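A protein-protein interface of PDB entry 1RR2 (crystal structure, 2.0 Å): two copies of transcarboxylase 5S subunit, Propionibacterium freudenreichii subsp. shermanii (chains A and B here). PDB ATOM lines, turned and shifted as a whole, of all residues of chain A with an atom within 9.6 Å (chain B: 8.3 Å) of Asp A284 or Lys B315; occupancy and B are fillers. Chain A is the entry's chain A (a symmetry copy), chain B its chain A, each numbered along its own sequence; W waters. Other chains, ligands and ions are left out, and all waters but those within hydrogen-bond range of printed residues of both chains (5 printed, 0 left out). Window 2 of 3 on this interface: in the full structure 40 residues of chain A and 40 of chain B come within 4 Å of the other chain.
The backbone NH (N) of Asp A284 sits at hydrogen-bond distance from the side-chain carboxylate (OD1) of Asp A282 (2.9 Å).
Of the printed residues of chain B, Glu A266 touches Thr B311 (3.5 Å).
Of the printed residues of chain B, Glu A270 touches Lys B202 (2.9 Å) and Phe B314 (3.7 Å).
Tyr A283 touches none of the printed residues of chain B.
Asp A284 touches just one residue of chain B: Lys B315 (3.8 Å).
Of the printed residues of chain A, Lys B202 touches Glu A270 (2.9 Å) and Glu A273 (2.6 Å).
Lys B315 touches just one residue of chain A: Asp A284.
Gln B317 touches none of the printed residues of chain A.
The nearest printed residue of chain A that does not touch Thr B311 is Glu A270 (4.2 Å).
Water W5 bridges OG1 of Thr B311 (2.6 Å) and OE2 of Glu A270 (2.8 Å).
Water W1 lies within hydrogen-bond range of N of Thr B311 (2.9 Å) and NE of Arg A290 (3.5 Å).
Water W4 lies within hydrogen-bond range of the backbone carbonyl oxygen (O) of Thr B311 (3.0 Å), the side-chain carboxylate (OE2) of Glu A270 (3.3 Å) and the backbone NH (N) of Lys B315 (3.4 Å).
Water W3 bridges the side-chain amino group of Lys B315 and the side-chain carboxylate of Asp A284.
Water W2 lies within hydrogen-bond range of the side-chain carboxylate (OE1) of Glu A270 (3.1 Å), the side-chain hydroxyl (OH) of Tyr A283 (3.1 Å) and the side-chain amino group (NZ) of Lys B202 (3.3 Å).
Among the printed residues, merely in contact across the chains: Glu A266 with Thr B311 (3.5 Å) and Glu A270 with Phe B314 (3.7 Å).
Hydrophobic or aromatic side chains of chain B that line the printed part of chain A: Phe B314.
Among the printed residues, Asp or Glu carboxylates within 4 Å of a Lys or Arg side-chain nitrogen of the other chain: Glu A270 with Lys B202, Glu A273 with Lys B202 and Asp A284 with Lys B315.
The side-chain carboxylate (OE1) of Glu A270 is in salt-bridge range of the side-chain amino group (NZ) of Lys B202 (2.9 Å).
The side-chain amino group (NZ) of Lys B202 lies within salt-bridge range of the side-chain carboxylate (OE1) of Glu A273.
The side-chain amino group (NZ) of Lys B315 lies within salt-bridge range of the side-chain carboxylate (OD2) of Asp A284 (3.8 Å).
No position is printed for both chains.
Of the 5 pairs that touch across the chains among the printed residues, none has its exchanged pair printed and touching as well.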
ATOM      1  N   ASP A  55      -9.083  -5.079   1.257  1.00  0.00           N
ATOM      2  CA  ASP A  55     -10.212  -4.297   0.735  1.00  0.00           C
ATOM      3  C   ASP A  55      -9.773  -2.867   0.421  1.00  0.00           C
ATOM      4  O   ASP A  55     -10.194  -2.287  -0.583  1.00  0.00           O
ATOM      5  CB  ASP A  55     -11.361  -4.309   1.734  1.00  0.00           C
ATOM      6  CG  ASP A  55     -12.024  -5.679   1.826  1.00  0.00           C
ATOM      7  OD1 ASP A  55     -12.347  -6.248   0.750  1.00  0.00           O
ATOM      8  OD2 ASP A  55     -12.221  -6.175   2.959  1.00  0.00           O
ATOM      9  N   ILE A  56      -8.920  -2.300   1.265  1.00  0.00           N
ATOM     10  CA  ILE A  56      -8.438  -0.929   1.038  1.00  0.00           C
ATOM     11  C   ILE A  56      -7.659  -0.872  -0.277  1.00  0.00           C
ATOM     12  O   ILE A  56      -7.800   0.070  -1.062  1.00  0.00           O
ATOM     13  CB  ILE A  56      -7.531  -0.486   2.205  1.00  0.00           C
ATOM     14  CG1 ILE A  56      -8.406  -0.078   3.399  1.00  0.00           C
ATOM     15  CG2 ILE A  56      -6.611   0.664   1.770  1.00  0.00           C
ATOM     16  CD1 ILE A  56      -7.625   0.196   4.664  1.00  0.00           C
ATOM     17  N   ALA A  58      -8.073  -2.663  -2.865  1.00  0.00           N
ATOM     18  CA  ALA A  58      -8.915  -2.859  -4.053  1.00  0.00           C
ATOM     19  C   ALA A  58     -10.066  -1.849  -4.086  1.00  0.00           C
ATOM     20  O   ALA A  58     -10.958  -1.980  -4.914  1.00  0.00           O
ATOM     21  CB  ALA A  58      -9.484  -4.290  -4.058  1.00  0.00           C
ATOM     22  N   ALA A  59     -10.045  -0.835  -3.229  1.00  0.00           N
ATOM     23  CA  ALA A  59     -11.170   0.111  -3.175  1.00  0.00           C
ATOM     24  C   ALA A  59     -11.160   1.102  -4.349  1.00  0.00           C
ATOM     25  O   ALA A  59     -12.224   1.505  -4.813  1.00  0.00           O
ATOM     26  CB  ALA A  59     -11.154   0.851  -1.842  1.00  0.00           C
ATOM     27  N   GLY A  60      -9.981   1.507  -4.821  1.00  0.00           N
ATOM     28  CA  GLY A  60      -9.920   2.448  -5.932  1.00  0.00           C
ATOM     29  C   GLY A  60      -9.377   3.820  -5.554  1.00  0.00           C
ATOM     30  O   GLY A  60      -9.531   4.791  -6.295  1.00  0.00           O
ATOM     31  N   TYR A  61      -8.709   3.895  -4.407  1.00  0.00           N
ATOM     32  CA  TYR A  61      -8.142   5.147  -3.886  1.00  0.00           C
ATOM     33  C   TYR A  61      -6.961   5.617  -4.724  1.00  0.00           C
ATOM     34  O   TYR A  61      -6.238   4.812  -5.305  1.00  0.00           O
ATOM     35  CB  TYR A  61      -7.640   4.930  -2.459  1.00  0.00           C
ATOM     36  CG  TYR A  61      -8.715   4.586  -1.471  1.00  0.00           C
ATOM     37  CD1 TYR A  61      -8.673   3.393  -0.754  1.00  0.00           C
ATOM     38  CD2 TYR A  61      -9.737   5.486  -1.188  1.00  0.00           C
ATOM     39  CE1 TYR A  61      -9.627   3.111   0.241  1.00  0.00           C
ATOM     40  CE2 TYR A  61     -10.687   5.218  -0.194  1.00  0.00           C
ATOM     41  CZ  TYR A  61     -10.624   4.037   0.520  1.00  0.00           C
ATOM     42  OH  TYR A  61     -11.509   3.811   1.559  1.00  0.00           O
ATOM     43  N   ILE A 253     -12.666   6.581   6.153  1.00  0.00           N
ATOM     44  CA  ILE A 253     -13.833   5.687   6.065  1.00  0.00           C
ATOM     45  C   ILE A 253     -14.887   6.163   7.126  1.00  0.00           C
ATOM     46  O   ILE A 253     -14.514   6.570   8.239  1.00  0.00           O
ATOM     47  CB  ILE A 253     -13.363   4.203   6.218  1.00  0.00           C
ATOM     48  CG1 ILE A 253     -14.365   3.233   5.565  1.00  0.00           C
ATOM     49  CG2 ILE A 253     -13.117   3.890   7.668  1.00  0.00           C
ATOM     50  CD1 ILE A 253     -14.519   3.383   4.031  1.00  0.00           C
ATOM     51  N   GLU A 266     -17.237   7.578   2.124  1.00  0.00           N
ATOM     52  CA  GLU A 266     -18.480   7.200   1.434  1.00  0.00           C
ATOM     53  C   GLU A 266     -19.379   8.422   1.199  1.00  0.00           C
ATOM     54  O   GLU A 266     -20.010   8.532   0.139  1.00  0.00           O
ATOM     55  CB  GLU A 266     -19.237   6.133   2.231  1.00  0.00           C
ATOM     56  CG  GLU A 266     -18.425   4.858   2.459  1.00  0.00           C
ATOM     57  CD  GLU A 266     -17.855   4.792   3.869  1.00  0.00           C
ATOM     58  OE1 GLU A 266     -17.063   5.682   4.253  1.00  0.00           O
ATOM     59  OE2 GLU A 266     -18.222   3.849   4.594  1.00  0.00           O
ATOM     60  N   GLU A 270     -20.642   9.622  -2.357  1.00  0.00           N
ATOM     61  CA  GLU A 270     -22.082   9.630  -2.661  1.00  0.00           C
ATOM     62  C   GLU A 270     -22.612  11.021  -3.047  1.00  0.00           C
ATOM     63  O   GLU A 270     -23.451  11.125  -3.938  1.00  0.00           O
ATOM     64  CB  GLU A 270     -22.881   9.112  -1.454  1.00  0.00           C
ATOM     65  CG  GLU A 270     -22.614   7.649  -1.097  1.00  0.00           C
ATOM     66  CD  GLU A 270     -23.428   6.666  -1.936  1.00  0.00           C
ATOM     67  OE1 GLU A 270     -24.034   7.082  -2.954  1.00  0.00           O
ATOM     68  OE2 GLU A 270     -23.458   5.465  -1.575  1.00  0.00           O
ATOM     69  N   GLU A 273     -23.057  12.289  -6.934  1.00  0.00           N
ATOM     70  CA  GLU A 273     -23.974  11.706  -7.926  1.00  0.00           C
ATOM     71  C   GLU A 273     -24.830  12.771  -8.602  1.00  0.00           C
ATOM     72  O   GLU A 273     -25.523  13.544  -7.943  1.00  0.00           O
ATOM     73  CB  GLU A 273     -24.881  10.643  -7.293  1.00  0.00           C
ATOM     74  CG  GLU A 273     -25.854  10.021  -8.297  1.00  0.00           C
ATOM     75  CD  GLU A 273     -26.606   8.818  -7.748  1.00  0.00           C
ATOM     76  OE1 GLU A 273     -26.713   8.692  -6.509  1.00  0.00           O
ATOM     77  OE2 GLU A 273     -27.103   8.005  -8.564  1.00  0.00           O
ATOM     78  N   ASN A 280     -13.870   6.897  -8.422  1.00  0.00           N
ATOM     79  CA  ASN A 280     -14.099   5.525  -8.885  1.00  0.00           C
ATOM     80  C   ASN A 280     -13.760   4.579  -7.758  1.00  0.00           C
ATOM     81  O   ASN A 280     -12.891   3.727  -7.885  1.00  0.00           O
ATOM     82  CB  ASN A 280     -13.308   5.168 -10.147  1.00  0.00           C
ATOM     83  CG  ASN A 280     -13.918   3.935 -10.808  1.00  0.00           C
ATOM     84  OD1 ASN A 280     -13.210   3.156 -11.444  1.00  0.00           O
ATOM     85  ND2 ASN A 280     -15.240   3.760 -10.684  1.00  0.00           N
ATOM     86  N   LEU A 281     -14.442   4.763  -6.634  1.00  0.00           N
ATOM     87  CA  LEU A 281     -14.254   3.859  -5.491  1.00  0.00           C
ATOM     88  C   LEU A 281     -15.289   2.759  -5.610  1.00  0.00           C
ATOM     89  O   LEU A 281     -16.350   2.972  -6.192  1.00  0.00           O
ATOM     90  CB  LEU A 281     -14.450   4.616  -4.169  1.00  0.00           C
ATOM     91  CG  LEU A 281     -13.527   5.818  -3.937  1.00  0.00           C
ATOM     92  CD1 LEU A 281     -13.812   6.433  -2.551  1.00  0.00           C
ATOM     93  CD2 LEU A 281     -12.065   5.358  -4.060  1.00  0.00           C
ATOM     94  N   ASP A 282     -14.961   1.585  -5.074  1.00  0.00           N
ATOM     95  CA  ASP A 282     -15.859   0.421  -5.082  1.00  0.00           C
ATOM     96  C   ASP A 282     -16.666   0.468  -3.781  1.00  0.00           C
ATOM     97  O   ASP A 282     -16.116   0.229  -2.700  1.00  0.00           O
ATOM     98  CB  ASP A 282     -15.001  -0.836  -5.142  1.00  0.00           C
ATOM     99  CG  ASP A 282     -15.814  -2.096  -5.233  1.00  0.00           C
ATOM    100  OD1 ASP A 282     -16.837  -2.188  -4.528  1.00  0.00           O
ATOM    101  OD2 ASP A 282     -15.412  -3.001  -5.993  1.00  0.00           O
ATOM    102  N   TYR A 283     -17.963   0.761  -3.877  1.00  0.00           N
ATOM    103  CA  TYR A 283     -18.803   0.908  -2.678  1.00  0.00           C
ATOM    104  C   TYR A 283     -18.826  -0.362  -1.827  1.00  0.00           C
ATOM    105  O   TYR A 283     -18.957  -0.283  -0.599  1.00  0.00           O
ATOM    106  CB  TYR A 283     -20.220   1.330  -3.064  1.00  0.00           C
ATOM    107  CG  TYR A 283     -20.320   2.791  -3.466  1.00  0.00           C
ATOM    108  CD1 TYR A 283     -20.445   3.163  -4.803  1.00  0.00           C
ATOM    109  CD2 TYR A 283     -20.257   3.802  -2.510  1.00  0.00           C
ATOM    110  CE1 TYR A 283     -20.505   4.509  -5.177  1.00  0.00           C
ATOM    111  CE2 TYR A 283     -20.314   5.149  -2.874  1.00  0.00           C
ATOM    112  CZ  TYR A 283     -20.437   5.494  -4.206  1.00  0.00           C
ATOM    113  OH  TYR A 283     -20.482   6.826  -4.569  1.00  0.00           O
ATOM    114  N   ASP A 284     -18.702  -1.520  -2.459  1.00  0.00           N
ATOM    115  CA  ASP A 284     -18.699  -2.786  -1.711  1.00  0.00           C
ATOM    116  C   ASP A 284     -17.443  -2.877  -0.870  1.00  0.00           C
ATOM    117  O   ASP A 284     -17.515  -3.218   0.302  1.00  0.00           O
ATOM    118  CB  ASP A 284     -18.779  -3.966  -2.663  1.00  0.00           C
ATOM    119  CG  ASP A 284     -20.202  -4.308  -3.012  1.00  0.00           C
ATOM    120  OD1 ASP A 284     -20.437  -4.842  -4.121  1.00  0.00           O
ATOM    121  OD2 ASP A 284     -21.087  -4.041  -2.164  1.00  0.00           O
ATOM    122  N   ARG A 285     -16.294  -2.576  -1.467  1.00  0.00           N
ATOM    123  CA  ARG A 285     -15.038  -2.609  -0.707  1.00  0.00           C
ATOM    124  C   ARG A 285     -15.143  -1.611   0.447  1.00  0.00           C
ATOM    125  O   ARG A 285     -14.781  -1.922   1.579  1.00  0.00           O
ATOM    126  CB  ARG A 285     -13.867  -2.235  -1.605  1.00  0.00           C
ATOM    127  CG  ARG A 285     -13.590  -3.213  -2.749  1.00  0.00           C
ATOM    128  CD  ARG A 285     -13.107  -4.575  -2.247  1.00  0.00           C
ATOM    129  NE  ARG A 285     -12.694  -5.573  -3.233  1.00  0.00           N
ATOM    130  CZ  ARG A 285     -11.983  -6.674  -2.995  1.00  0.00           C
ATOM    131  NH1 ARG A 285     -11.567  -6.991  -1.776  1.00  0.00           N
ATOM    132  NH2 ARG A 285     -11.641  -7.450  -4.011  1.00  0.00           N
ATOM    133  N   LEU A 286     -15.661  -0.423   0.162  1.00  0.00           N
ATOM    134  CA  LEU A 286     -15.798   0.609   1.202  1.00  0.00           C
ATOM    135  C   LEU A 286     -16.653   0.084   2.341  1.00  0.00           C
ATOM    136  O   LEU A 286     -16.351   0.308   3.504  1.00  0.00           O
ATOM    137  CB  LEU A 286     -16.449   1.872   0.636  1.00  0.00           C
ATOM    138  CG  LEU A 286     -15.668   2.630  -0.432  1.00  0.00           C
ATOM    139  CD1 LEU A 286     -16.412   3.910  -0.789  1.00  0.00           C
ATOM    140  CD2 LEU A 286     -14.258   2.957   0.080  1.00  0.00           C
ATOM    141  N   HIS A 287     -17.720  -0.626   2.005  1.00  0.00           N
ATOM    142  CA  HIS A 287     -18.624  -1.159   3.034  1.00  0.00           C
ATOM    143  C   HIS A 287     -17.871  -2.108   3.969  1.00  0.00           C
ATOM    144  O   HIS A 287     -18.081  -2.088   5.182  1.00  0.00           O
ATOM    145  CB  HIS A 287     -19.768  -1.903   2.377  1.00  0.00           C
ATOM    146  CG  HIS A 287     -20.803  -2.360   3.344  1.00  0.00           C
ATOM    147  ND1 HIS A 287     -21.760  -1.513   3.858  1.00  0.00           N
ATOM    148  CD2 HIS A 287     -21.005  -3.562   3.935  1.00  0.00           C
ATOM    149  CE1 HIS A 287     -22.510  -2.173   4.723  1.00  0.00           C
ATOM    150  NE2 HIS A 287     -22.072  -3.417   4.790  1.00  0.00           N
ATOM    151  N   LYS A 288     -17.001  -2.940   3.407  1.00  0.00           N
ATOM    152  CA  LYS A 288     -16.225  -3.905   4.203  1.00  0.00           C
ATOM    153  C   LYS A 288     -15.227  -3.175   5.088  1.00  0.00           C
ATOM    154  O   LYS A 288     -15.047  -3.524   6.251  1.00  0.00           O
ATOM    155  CB  LYS A 288     -15.479  -4.878   3.291  1.00  0.00           C
ATOM    156  CG  LYS A 288     -16.397  -5.712   2.396  1.00  0.00           C
ATOM    157  CD  LYS A 288     -15.581  -6.680   1.539  1.00  0.00           C
ATOM    158  CE  LYS A 288     -16.494  -7.510   0.634  1.00  0.00           C
ATOM    159  NZ  LYS A 288     -15.680  -8.342  -0.311  1.00  0.00           N
ATOM    160  N   ILE A 289     -14.565  -2.170   4.533  1.00  0.00           N
ATOM    161  CA  ILE A 289     -13.590  -1.393   5.310  1.00  0.00           C
ATOM    162  C   ILE A 289     -14.336  -0.695   6.455  1.00  0.00           C
ATOM    163  O   ILE A 289     -13.868  -0.660   7.598  1.00  0.00           O
ATOM    164  CB  ILE A 289     -12.909  -0.331   4.408  1.00  0.00           C
ATOM    165  CG1 ILE A 289     -12.244  -1.021   3.213  1.00  0.00           C
ATOM    166  CG2 ILE A 289     -11.866   0.444   5.201  1.00  0.00           C
ATOM    167  CD1 ILE A 289     -11.821  -0.051   2.091  1.00  0.00           C
ATOM    168  N   ARG A 290     -15.515  -0.160   6.153  1.00  0.00           N
ATOM    169  CA  ARG A 290     -16.310   0.541   7.173  1.00  0.00           C
ATOM    170  C   ARG A 290     -16.678  -0.421   8.310  1.00  0.00           C
ATOM    171  O   ARG A 290     -16.495  -0.106   9.484  1.00  0.00           O
ATOM    172  CB  ARG A 290     -17.604   1.092   6.577  1.00  0.00           C
ATOM    173  CG  ARG A 290     -18.447   1.810   7.633  1.00  0.00           C
ATOM    174  CD  ARG A 290     -19.809   2.227   7.076  1.00  0.00           C
ATOM    175  NE  ARG A 290     -20.826   1.222   6.801  1.00  0.00           N
ATOM    176  CZ  ARG A 290     -21.708   0.800   7.703  1.00  0.00           C
ATOM    177  NH1 ARG A 290     -21.683   1.309   8.935  1.00  0.00           N
ATOM    178  NH2 ARG A 290     -22.617  -0.124   7.378  1.00  0.00           N
ATOM    179  N   ASP A 291     -17.212  -1.580   7.954  1.00  0.00           N
ATOM    180  CA  ASP A 291     -17.626  -2.574   8.954  1.00  0.00           C
ATOM    181  C   ASP A 291     -16.409  -3.050   9.731  1.00  0.00           C
ATOM    182  O   ASP A 291     -16.479  -3.280  10.929  1.00  0.00           O
ATOM    183  CB  ASP A 291     -18.329  -3.752   8.265  1.00  0.00           C
ATOM    184  CG  ASP A 291     -19.730  -3.386   7.763  1.00  0.00           C
ATOM    185  OD1 ASP A 291     -20.230  -2.293   8.133  1.00  0.00           O
ATOM    186  OD2 ASP A 291     -20.333  -4.186   7.009  1.00  0.00           O
ATOM    187  N   HIS A 292     -15.278  -3.173   9.057  1.00  0.00           N
ATOM    188  CA  HIS A 292     -14.068  -3.628   9.756  1.00  0.00           C
ATOM    189  C   HIS A 292     -13.745  -2.694  10.925  1.00  0.00           C
ATOM    190  O   HIS A 292     -13.634  -3.137  12.069  1.00  0.00           O
ATOM    191  CB  HIS A 292     -12.877  -3.662   8.810  1.00  0.00           C
ATOM    192  CG  HIS A 292     -11.614  -4.090   9.480  1.00  0.00           C
ATOM    193  ND1 HIS A 292     -11.308  -5.414   9.701  1.00  0.00           N
ATOM    194  CD2 HIS A 292     -10.637  -3.371  10.081  1.00  0.00           C
ATOM    195  CE1 HIS A 292     -10.199  -5.494  10.414  1.00  0.00           C
ATOM    196  NE2 HIS A 292      -9.772  -4.268  10.659  1.00  0.00           N
ATOM    197  N   ILE B 168     -36.402   8.460  -2.212  1.00  0.00           N
ATOM    198  CA  ILE B 168     -35.865   8.035  -3.513  1.00  0.00           C
ATOM    199  C   ILE B 168     -36.583   6.758  -3.915  1.00  0.00           C
ATOM    200  O   ILE B 168     -36.628   5.803  -3.142  1.00  0.00           O
ATOM    201  CB  ILE B 168     -34.342   7.783  -3.468  1.00  0.00           C
ATOM    202  CG1 ILE B 168     -33.605   9.113  -3.300  1.00  0.00           C
ATOM    203  CG2 ILE B 168     -33.881   7.129  -4.780  1.00  0.00           C
ATOM    204  CD1 ILE B 168     -32.115   8.977  -2.975  1.00  0.00           C
ATOM    205  N   LEU B 200     -31.652  11.489   2.624  1.00  0.00           N
ATOM    206  CA  LEU B 200     -31.525  10.902   1.282  1.00  0.00           C
ATOM    207  C   LEU B 200     -31.279  11.965   0.216  1.00  0.00           C
ATOM    208  O   LEU B 200     -30.895  11.615  -0.909  1.00  0.00           O
ATOM    209  CB  LEU B 200     -32.814  10.157   0.910  1.00  0.00           C
ATOM    210  CG  LEU B 200     -33.051   8.759   1.473  1.00  0.00           C
ATOM    211  CD1 LEU B 200     -34.494   8.343   1.280  1.00  0.00           C
ATOM    212  CD2 LEU B 200     -32.092   7.806   0.781  1.00  0.00           C
ATOM    213  N   LYS B 202     -29.472  14.346  -1.954  1.00  0.00           N
ATOM    214  CA  LYS B 202     -28.099  14.658  -2.372  1.00  0.00           C
ATOM    215  C   LYS B 202     -28.057  16.090  -2.912  1.00  0.00           C
ATOM    216  O   LYS B 202     -29.100  16.697  -3.160  1.00  0.00           O
ATOM    217  CB  LYS B 202     -27.591  13.647  -3.414  1.00  0.00           C
ATOM    218  CG  LYS B 202     -27.336  12.250  -2.844  1.00  0.00           C
ATOM    219  CD  LYS B 202     -26.742  11.319  -3.905  1.00  0.00           C
ATOM    220  CE  LYS B 202     -26.417   9.946  -3.315  1.00  0.00           C
ATOM    221  NZ  LYS B 202     -25.570   9.129  -4.239  1.00  0.00           N
ATOM    222  N   THR B 311     -24.250   5.526   5.039  1.00  0.00           N
ATOM    223  CA  THR B 311     -24.676   5.789   3.657  1.00  0.00           C
ATOM    224  C   THR B 311     -25.305   4.534   3.025  1.00  0.00           C
ATOM    225  O   THR B 311     -25.651   4.546   1.838  1.00  0.00           O
ATOM    226  CB  THR B 311     -23.465   6.162   2.770  1.00  0.00           C
ATOM    227  OG1 THR B 311     -22.508   5.096   2.799  1.00  0.00           O
ATOM    228  CG2 THR B 311     -22.783   7.420   3.267  1.00  0.00           C
ATOM    229  N   SER B 312     -25.465   3.466   3.799  1.00  0.00           N
ATOM    230  CA  SER B 312     -25.994   2.209   3.248  1.00  0.00           C
ATOM    231  C   SER B 312     -27.395   2.387   2.660  1.00  0.00           C
ATOM    232  O   SER B 312     -27.778   1.633   1.770  1.00  0.00           O
ATOM    233  CB  SER B 312     -26.007   1.111   4.315  1.00  0.00           C
ATOM    234  OG  SER B 312     -26.865   1.441   5.386  1.00  0.00           O
ATOM    235  N   ILE B 313     -28.156   3.372   3.122  1.00  0.00           N
ATOM    236  CA  ILE B 313     -29.523   3.559   2.611  1.00  0.00           C
ATOM    237  C   ILE B 313     -29.520   3.905   1.108  1.00  0.00           C
ATOM    238  O   ILE B 313     -30.493   3.634   0.406  1.00  0.00           O
ATOM    239  CB  ILE B 313     -30.269   4.663   3.402  1.00  0.00           C
ATOM    240  CG1 ILE B 313     -31.743   4.698   2.976  1.00  0.00           C
ATOM    241  CG2 ILE B 313     -29.615   6.026   3.173  1.00  0.00           C
ATOM    242  CD1 ILE B 313     -32.620   5.677   3.787  1.00  0.00           C
ATOM    243  N   PHE B 314     -28.443   4.497   0.600  1.00  0.00           N
ATOM    244  CA  PHE B 314     -28.400   4.856  -0.825  1.00  0.00           C
ATOM    245  C   PHE B 314     -28.411   3.601  -1.694  1.00  0.00           C
ATOM    246  O   PHE B 314     -28.655   3.678  -2.895  1.00  0.00           O
ATOM    247  CB  PHE B 314     -27.161   5.697  -1.137  1.00  0.00           C
ATOM    248  CG  PHE B 314     -27.252   7.102  -0.617  1.00  0.00           C
ATOM    249  CD1 PHE B 314     -26.248   7.633   0.190  1.00  0.00           C
ATOM    250  CD2 PHE B 314     -28.351   7.901  -0.942  1.00  0.00           C
ATOM    251  CE1 PHE B 314     -26.335   8.944   0.665  1.00  0.00           C
ATOM    252  CE2 PHE B 314     -28.449   9.214  -0.473  1.00  0.00           C
ATOM    253  CZ  PHE B 314     -27.439   9.738   0.332  1.00  0.00           C
ATOM    254  N   LYS B 315     -28.147   2.455  -1.083  1.00  0.00           N
ATOM    255  CA  LYS B 315     -28.135   1.179  -1.811  1.00  0.00           C
ATOM    256  C   LYS B 315     -29.334   0.309  -1.414  1.00  0.00           C
ATOM    257  O   LYS B 315     -29.949  -0.320  -2.263  1.00  0.00           O
ATOM    258  CB  LYS B 315     -26.868   0.389  -1.491  1.00  0.00           C
ATOM    259  CG  LYS B 315     -26.929  -1.037  -2.046  1.00  0.00           C
ATOM    260  CD  LYS B 315     -25.773  -1.902  -1.541  1.00  0.00           C
ATOM    261  CE  LYS B 315     -25.874  -3.320  -2.111  1.00  0.00           C
ATOM    262  NZ  LYS B 315     -24.809  -4.247  -1.621  1.00  0.00           N
ATOM    263  N   SER B 316     -29.668   0.295  -0.129  1.00  0.00           N
ATOM    264  CA  SER B 316     -30.717  -0.587   0.400  1.00  0.00           C
ATOM    265  C   SER B 316     -32.105   0.055   0.453  1.00  0.00           C
ATOM    266  O   SER B 316     -33.099  -0.675   0.532  1.00  0.00           O
ATOM    267  CB  SER B 316     -30.342  -1.003   1.812  1.00  0.00           C
ATOM    268  OG  SER B 316     -30.419   0.124   2.674  1.00  0.00           O
ATOM    269  N   GLN B 317     -32.194   1.380   0.424  1.00  0.00           N
ATOM    270  CA  GLN B 317     -33.493   2.060   0.549  1.00  0.00           C
ATOM    271  C   GLN B 317     -34.033   1.855   1.964  1.00  0.00           C
ATOM    272  O   GLN B 317     -35.123   2.330   2.273  1.00  0.00           O
ATOM    273  CB  GLN B 317     -34.572   1.485  -0.362  1.00  0.00           C
ATOM    274  CG  GLN B 317     -34.417   1.593  -1.879  1.00  0.00           C
ATOM    275  CD  GLN B 317     -35.600   0.910  -2.564  1.00  0.00           C
ATOM    276  OE1 GLN B 317     -36.766   1.314  -2.385  1.00  0.00           O
ATOM    277  NE2 GLN B 317     -35.308  -0.146  -3.335  1.00  0.00           N
ATOM    278  N   ILE B 318     -33.302   1.148   2.819  1.00  0.00           N
ATOM    279  CA  ILE B 318     -33.810   0.886   4.173  1.00  0.00           C
ATOM    280  C   ILE B 318     -33.122   1.779   5.196  1.00  0.00           C
ATOM    281  O   ILE B 318     -31.904   1.739   5.338  1.00  0.00           O
ATOM    282  CB  ILE B 318     -33.566  -0.582   4.592  1.00  0.00           C
ATOM    283  CG1 ILE B 318     -34.181  -1.539   3.572  1.00  0.00           C
ATOM    284  CG2 ILE B 318     -34.167  -0.835   5.970  1.00  0.00           C
ATOM    285  CD1 ILE B 318     -33.817  -3.009   3.817  1.00  0.00           C
ATOM    286  N   MET B 343     -34.200  -7.923   3.596  1.00  0.00           N
ATOM    287  CA  MET B 343     -33.769  -6.670   2.959  1.00  0.00           C
ATOM    288  C   MET B 343     -34.077  -6.705   1.467  1.00  0.00           C
ATOM    289  O   MET B 343     -34.247  -5.663   0.835  1.00  0.00           O
ATOM    290  CB  MET B 343     -32.269  -6.432   3.177  1.00  0.00           C
ATOM    291  CG  MET B 343     -31.890  -6.115   4.626  1.00  0.00           C
ATOM    292  SD  MET B 343     -30.105  -6.016   4.902  1.00  0.00           S
ATOM    293  CE  MET B 343     -29.601  -4.841   3.622  1.00  0.00           C
ATOM    294  N   PRO B 347     -37.942  -3.918  -0.728  1.00  0.00           N
ATOM    295  CA  PRO B 347     -38.235  -3.244  -1.997  1.00  0.00           C
ATOM    296  C   PRO B 347     -39.518  -3.740  -2.647  1.00  0.00           C
ATOM    297  O   PRO B 347     -40.323  -2.952  -3.135  1.00  0.00           O
ATOM    298  CB  PRO B 347     -37.010  -3.563  -2.845  1.00  0.00           C
ATOM    299  CG  PRO B 347     -35.912  -3.584  -1.822  1.00  0.00           C
ATOM    300  CD  PRO B 347     -36.537  -4.363  -0.683  1.00  0.00           C
HETATM  301  O   HOH W   1     -21.587   4.428   5.637  1.00  0.00           O
HETATM  302  O   HOH W   2     -23.180   7.449  -5.861  1.00  0.00           O
HETATM  303  O   HOH W   3     -22.786  -3.476   0.390  1.00  0.00           O
HETATM  304  O   HOH W   4     -24.881   2.711  -0.347  1.00  0.00           O
HETATM  305  O   HOH W   5     -21.702   4.415   0.402  1.00  0.00           O
